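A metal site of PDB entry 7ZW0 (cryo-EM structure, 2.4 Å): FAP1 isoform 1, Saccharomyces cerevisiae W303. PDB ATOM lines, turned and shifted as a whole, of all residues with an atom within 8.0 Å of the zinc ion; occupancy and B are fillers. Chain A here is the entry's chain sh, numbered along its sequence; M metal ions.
The backbone carbonyl oxygen (O) of Pro 405 lies close to the side-chain sulfur (SG) of Cys 388 (2.9 Å). The backbone NH (N) of Cys 388 is in hydrogen-bond range of the backbone carbonyl oxygen (O) of Ser 393, 2.9 Å away. NH2 of Arg 406 sits at hydrogen-bond distance from O of Cys 426. The backbone NH (N) of Cys 426 is in hydrogen-bond range of the backbone carbonyl oxygen (O) of Ile 409 (3.1 Å). The side-chain sulfur of Cys 426 sits close to the backbone carbonyl oxygen of Pro 405 (3.5 Å).
Four residues have an atom within 4 Å of the zinc ion: Cys 388, Cys 390, Cys 407 and Cys 426.
The zinc ion is bound by SG of Cys 407 (2.2 Å). The side-chain sulfur (SG) of Cys 388 binds the zinc ion, 2.3 Å away. The side-chain sulfur (SG) of Cys 426 is bound to the zinc ion (2.3 Å). SG of Cys 390 is bound to the zinc ion.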
ATOM      1  N   LYS A 387      31.643  29.558  16.204  1.00  0.00           N
ATOM      2  CA  LYS A 387      30.230  29.287  16.467  1.00  0.00           C
ATOM      3  C   LYS A 387      29.999  28.469  17.722  1.00  0.00           C
ATOM      4  O   LYS A 387      30.794  27.583  18.045  1.00  0.00           O
ATOM      5  CB  LYS A 387      29.582  28.610  15.254  1.00  0.00           C
ATOM      6  CG  LYS A 387      29.625  29.451  13.997  1.00  0.00           C
ATOM      7  CD  LYS A 387      28.636  28.953  12.957  1.00  0.00           C
ATOM      8  CE  LYS A 387      28.643  29.850  11.723  1.00  0.00           C
ATOM      9  NZ  LYS A 387      27.692  29.375  10.681  1.00  0.00           N
ATOM     10  N   CYS A 388      28.919  28.760  18.442  1.00  0.00           N
ATOM     11  CA  CYS A 388      28.603  28.035  19.664  1.00  0.00           C
ATOM     12  C   CYS A 388      28.161  26.603  19.416  1.00  0.00           C
ATOM     13  O   CYS A 388      27.896  26.225  18.272  1.00  0.00           O
ATOM     14  CB  CYS A 388      27.520  28.777  20.460  1.00  0.00           C
ATOM     15  SG  CYS A 388      27.122  28.005  22.045  1.00  0.00           S
ATOM     16  N   ALA A 389      28.096  25.794  20.472  1.00  0.00           N
ATOM     17  CA  ALA A 389      27.681  24.397  20.327  1.00  0.00           C
ATOM     18  C   ALA A 389      26.273  24.373  19.752  1.00  0.00           C
ATOM     19  O   ALA A 389      25.957  23.523  18.921  1.00  0.00           O
ATOM     20  CB  ALA A 389      27.711  23.703  21.680  1.00  0.00           C
ATOM     21  N   CYS A 390      25.421  25.296  20.191  1.00  0.00           N
ATOM     22  CA  CYS A 390      24.088  25.405  19.609  1.00  0.00           C
ATOM     23  C   CYS A 390      24.234  25.741  18.140  1.00  0.00           C
ATOM     24  O   CYS A 390      23.366  25.353  17.353  1.00  0.00           O
ATOM     25  CB  CYS A 390      23.269  26.481  20.333  1.00  0.00           C
ATOM     26  SG  CYS A 390      23.034  26.183  22.098  1.00  0.00           S
ATOM     27  N   GLU A 391      25.278  26.489  17.784  1.00  0.00           N
ATOM     28  CA  GLU A 391      25.542  26.896  16.391  1.00  0.00           C
ATOM     29  C   GLU A 391      24.629  28.033  15.953  1.00  0.00           C
ATOM     30  O   GLU A 391      24.969  28.783  15.046  1.00  0.00           O
ATOM     31  CB  GLU A 391      25.516  25.718  15.392  1.00  0.00           C
ATOM     32  CG  GLU A 391      26.586  24.675  15.633  1.00  0.00           C
ATOM     33  CD  GLU A 391      27.948  25.093  15.118  1.00  0.00           C
ATOM     34  OE1 GLU A 391      28.967  24.645  15.686  1.00  0.00           O
ATOM     35  OE2 GLU A 391      28.003  25.857  14.137  1.00  0.00           O
ATOM     36  N   GLN A 392      23.467  28.159  16.597  1.00  0.00           N
ATOM     37  CA  GLN A 392      22.583  29.290  16.317  1.00  0.00           C
ATOM     38  C   GLN A 392      23.238  30.658  16.502  1.00  0.00           C
ATOM     39  O   GLN A 392      22.669  31.686  16.136  1.00  0.00           O
ATOM     40  CB  GLN A 392      21.327  29.216  17.210  1.00  0.00           C
ATOM     41  CG  GLN A 392      20.486  27.944  17.021  1.00  0.00           C
ATOM     42  CD  GLN A 392      20.079  27.711  15.573  1.00  0.00           C
ATOM     43  OE1 GLN A 392      19.679  28.599  14.856  1.00  0.00           O
ATOM     44  NE2 GLN A 392      20.194  26.495  15.085  1.00  0.00           N
ATOM     45  N   SER A 393      24.418  30.716  17.117  1.00  0.00           N
ATOM     46  CA  SER A 393      25.084  31.983  17.416  1.00  0.00           C
ATOM     47  C   SER A 393      26.576  31.883  17.212  1.00  0.00           C
ATOM     48  O   SER A 393      27.172  30.815  17.342  1.00  0.00           O
ATOM     49  CB  SER A 393      24.789  32.446  18.841  1.00  0.00           C
ATOM     50  OG  SER A 393      23.406  32.352  19.147  1.00  0.00           O
ATOM     51  N   PHE A 395      30.221  33.643  18.283  1.00  0.00           N
ATOM     52  CA  PHE A 395      30.910  34.565  19.154  1.00  0.00           C
ATOM     53  C   PHE A 395      32.336  34.734  18.663  1.00  0.00           C
ATOM     54  O   PHE A 395      33.064  33.752  18.537  1.00  0.00           O
ATOM     55  CB  PHE A 395      30.894  34.065  20.592  1.00  0.00           C
ATOM     56  CG  PHE A 395      29.524  33.952  21.188  1.00  0.00           C
ATOM     57  CD1 PHE A 395      28.950  35.031  21.832  1.00  0.00           C
ATOM     58  CD2 PHE A 395      28.801  32.780  21.091  1.00  0.00           C
ATOM     59  CE1 PHE A 395      27.676  34.935  22.377  1.00  0.00           C
ATOM     60  CE2 PHE A 395      27.539  32.673  21.631  1.00  0.00           C
ATOM     61  CZ  PHE A 395      26.974  33.754  22.271  1.00  0.00           C
ATOM     62  N   ARG A 404      34.880  27.033  24.882  1.00  0.00           N
ATOM     63  CA  ARG A 404      33.944  26.872  23.779  1.00  0.00           C
ATOM     64  C   ARG A 404      32.884  27.926  24.084  1.00  0.00           C
ATOM     65  O   ARG A 404      32.487  28.083  25.236  1.00  0.00           O
ATOM     66  CB  ARG A 404      33.328  25.476  23.787  1.00  0.00           C
ATOM     67  CG  ARG A 404      32.723  25.043  22.464  1.00  0.00           C
ATOM     68  CD  ARG A 404      31.669  23.970  22.661  1.00  0.00           C
ATOM     69  NE  ARG A 404      32.130  22.902  23.534  1.00  0.00           N
ATOM     70  CZ  ARG A 404      31.399  21.846  23.880  1.00  0.00           C
ATOM     71  NH1 ARG A 404      31.894  20.921  24.687  1.00  0.00           N
ATOM     72  NH2 ARG A 404      30.160  21.727  23.424  1.00  0.00           N
ATOM     73  N   PRO A 405      32.430  28.659  23.061  1.00  0.00           N
ATOM     74  CA  PRO A 405      31.484  29.755  23.345  1.00  0.00           C
ATOM     75  C   PRO A 405      30.169  29.284  23.932  1.00  0.00           C
ATOM     76  O   PRO A 405      29.651  28.239  23.539  1.00  0.00           O
ATOM     77  CB  PRO A 405      31.255  30.378  21.959  1.00  0.00           C
ATOM     78  CG  PRO A 405      31.641  29.319  20.989  1.00  0.00           C
ATOM     79  CD  PRO A 405      32.771  28.584  21.638  1.00  0.00           C
ATOM     80  N   ARG A 406      29.621  30.048  24.874  1.00  0.00           N
ATOM     81  CA  ARG A 406      28.374  29.667  25.514  1.00  0.00           C
ATOM     82  C   ARG A 406      27.261  30.663  25.200  1.00  0.00           C
ATOM     83  O   ARG A 406      27.452  31.870  25.365  1.00  0.00           O
ATOM     84  CB  ARG A 406      28.562  29.563  27.030  1.00  0.00           C
ATOM     85  CG  ARG A 406      29.717  28.683  27.477  1.00  0.00           C
ATOM     86  CD  ARG A 406      29.268  27.265  27.790  1.00  0.00           C
ATOM     87  NE  ARG A 406      28.890  26.508  26.605  1.00  0.00           N
ATOM     88  CZ  ARG A 406      29.709  25.704  25.938  1.00  0.00           C
ATOM     89  NH1 ARG A 406      30.960  25.524  26.349  1.00  0.00           N
ATOM     90  NH2 ARG A 406      29.276  25.058  24.868  1.00  0.00           N
ATOM     91  N   CYS A 407      26.114  30.171  24.759  1.00  0.00           N
ATOM     92  CA  CYS A 407      24.981  31.057  24.488  1.00  0.00           C
ATOM     93  C   CYS A 407      23.830  30.692  25.395  1.00  0.00           C
ATOM     94  O   CYS A 407      23.476  29.521  25.512  1.00  0.00           O
ATOM     95  CB  CYS A 407      24.555  30.981  23.014  1.00  0.00           C
ATOM     96  SG  CYS A 407      23.799  29.416  22.546  1.00  0.00           S
ATOM     97  N   ASN A 408      23.239  31.679  26.048  1.00  0.00           N
ATOM     98  CA  ASN A 408      22.164  31.408  27.004  1.00  0.00           C
ATOM     99  C   ASN A 408      20.872  30.913  26.364  1.00  0.00           C
ATOM    100  O   ASN A 408      19.919  31.682  26.247  1.00  0.00           O
ATOM    101  CB  ASN A 408      21.880  32.651  27.855  1.00  0.00           C
ATOM    102  CG  ASN A 408      23.083  33.084  28.660  1.00  0.00           C
ATOM    103  OD1 ASN A 408      23.046  34.105  29.358  1.00  0.00           O
ATOM    104  ND2 ASN A 408      24.166  32.324  28.571  1.00  0.00           N
ATOM    105  N   ILE A 409      20.832  29.649  25.954  1.00  0.00           N
ATOM    106  CA  ILE A 409      19.601  29.088  25.412  1.00  0.00           C
ATOM    107  C   ILE A 409      19.615  27.666  25.897  1.00  0.00           C
ATOM    108  O   ILE A 409      20.677  27.069  26.077  1.00  0.00           O
ATOM    109  CB  ILE A 409      19.529  29.147  23.876  1.00  0.00           C
ATOM    110  CG1 ILE A 409      18.084  29.012  23.405  1.00  0.00           C
ATOM    111  CG2 ILE A 409      20.425  28.105  23.218  1.00  0.00           C
ATOM    112  CD1 ILE A 409      17.161  30.063  23.959  1.00  0.00           C
ATOM    113  N   LYS A 410      18.444  27.115  26.134  1.00  0.00           N
ATOM    114  CA  LYS A 410      18.423  25.774  26.687  1.00  0.00           C
ATOM    115  C   LYS A 410      18.624  24.709  25.629  1.00  0.00           C
ATOM    116  O   LYS A 410      18.204  24.885  24.488  1.00  0.00           O
ATOM    117  CB  LYS A 410      17.125  25.525  27.463  1.00  0.00           C
ATOM    118  CG  LYS A 410      16.368  26.798  27.790  1.00  0.00           C
ATOM    119  CD  LYS A 410      15.771  26.730  29.192  1.00  0.00           C
ATOM    120  CE  LYS A 410      16.862  26.770  30.244  1.00  0.00           C
ATOM    121  NZ  LYS A 410      16.319  26.672  31.623  1.00  0.00           N
ATOM    122  N   CYS A 411      19.278  23.628  26.004  1.00  0.00           N
ATOM    123  CA  CYS A 411      19.506  22.522  25.082  1.00  0.00           C
ATOM    124  C   CYS A 411      18.226  22.032  24.421  1.00  0.00           C
ATOM    125  O   CYS A 411      18.213  21.802  23.223  1.00  0.00           O
ATOM    126  CB  CYS A 411      20.137  21.355  25.850  1.00  0.00           C
ATOM    127  SG  CYS A 411      20.387  19.849  24.896  1.00  0.00           S
ATOM    128  N   ASP A 424      19.728  22.051  30.128  1.00  0.00           N
ATOM    129  CA  ASP A 424      21.044  22.661  30.289  1.00  0.00           C
ATOM    130  C   ASP A 424      21.345  23.710  29.245  1.00  0.00           C
ATOM    131  O   ASP A 424      21.096  23.499  28.059  1.00  0.00           O
ATOM    132  CB  ASP A 424      22.131  21.583  30.275  1.00  0.00           C
ATOM    133  CG  ASP A 424      21.980  20.596  31.414  1.00  0.00           C
ATOM    134  OD1 ASP A 424      21.195  20.871  32.350  1.00  0.00           O
ATOM    135  OD2 ASP A 424      22.646  19.535  31.379  1.00  0.00           O
ATOM    136  N   ARG A 425      21.914  24.830  29.668  1.00  0.00           N
ATOM    137  CA  ARG A 425      22.249  25.921  28.747  1.00  0.00           C
ATOM    138  C   ARG A 425      23.508  25.656  27.938  1.00  0.00           C
ATOM    139  O   ARG A 425      24.557  25.367  28.513  1.00  0.00           O
ATOM    140  CB  ARG A 425      22.442  27.219  29.537  1.00  0.00           C
ATOM    141  CG  ARG A 425      21.609  28.392  29.046  1.00  0.00           C
ATOM    142  CD  ARG A 425      20.134  28.112  29.244  1.00  0.00           C
ATOM    143  NE  ARG A 425      19.287  29.112  28.601  1.00  0.00           N
ATOM    144  CZ  ARG A 425      18.769  30.168  29.228  1.00  0.00           C
ATOM    145  NH1 ARG A 425      19.011  30.356  30.510  1.00  0.00           N
ATOM    146  NH2 ARG A 425      18.015  31.032  28.562  1.00  0.00           N
ATOM    147  N   CYS A 426      23.409  25.744  26.608  1.00  0.00           N
ATOM    148  CA  CYS A 426      24.569  25.512  25.727  1.00  0.00           C
ATOM    149  C   CYS A 426      25.203  24.169  26.055  1.00  0.00           C
ATOM    150  O   CYS A 426      26.425  24.058  26.144  1.00  0.00           O
ATOM    151  CB  CYS A 426      25.582  26.652  25.772  1.00  0.00           C
ATOM    152  SG  CYS A 426      26.496  26.846  24.223  1.00  0.00           S
ATOM    153  N   CYS A 427      24.376  23.162  26.242  1.00  0.00           N
ATOM    154  CA  CYS A 427      24.845  21.843  26.620  1.00  0.00           C
ATOM    155  C   CYS A 427      25.895  21.197  25.705  1.00  0.00           C
ATOM    156  O   CYS A 427      25.795  21.305  24.484  1.00  0.00           O
ATOM    157  CB  CYS A 427      23.601  20.971  26.665  1.00  0.00           C
ATOM    158  SG  CYS A 427      23.837  19.256  27.073  1.00  0.00           S
ATOM    159  N   ARG A 430      24.260  18.670  23.282  1.00  0.00           N
ATOM    160  CA  ARG A 430      23.388  19.083  22.176  1.00  0.00           C
ATOM    161  C   ARG A 430      23.914  18.971  20.739  1.00  0.00           C
ATOM    162  O   ARG A 430      23.197  18.507  19.871  1.00  0.00           O
ATOM    163  CB  ARG A 430      22.859  20.515  22.426  1.00  0.00           C
ATOM    164  CG  ARG A 430      22.129  21.119  21.244  1.00  0.00           C
ATOM    165  CD  ARG A 430      21.190  22.242  21.655  1.00  0.00           C
ATOM    166  NE  ARG A 430      20.495  22.835  20.519  1.00  0.00           N
ATOM    167  CZ  ARG A 430      19.365  22.361  20.000  1.00  0.00           C
ATOM    168  NH1 ARG A 430      18.784  21.289  20.519  1.00  0.00           N
ATOM    169  NH2 ARG A 430      18.803  22.969  18.966  1.00  0.00           N
ATOM    170  N   PRO A 431      25.180  19.347  20.486  1.00  0.00           N
ATOM    171  CA  PRO A 431      25.610  19.188  19.087  1.00  0.00           C
ATOM    172  C   PRO A 431      25.565  17.728  18.676  1.00  0.00           C
ATOM    173  O   PRO A 431      25.137  17.413  17.558  1.00  0.00           O
ATOM    174  CB  PRO A 431      27.051  19.700  19.093  1.00  0.00           C
ATOM    175  CG  PRO A 431      27.456  19.738  20.523  1.00  0.00           C
ATOM    176  CD  PRO A 431      26.206  20.069  21.264  1.00  0.00           C
HETATM  177 ZN    ZN M   1      24.981  27.581  22.631  1.00  0.00          ZN
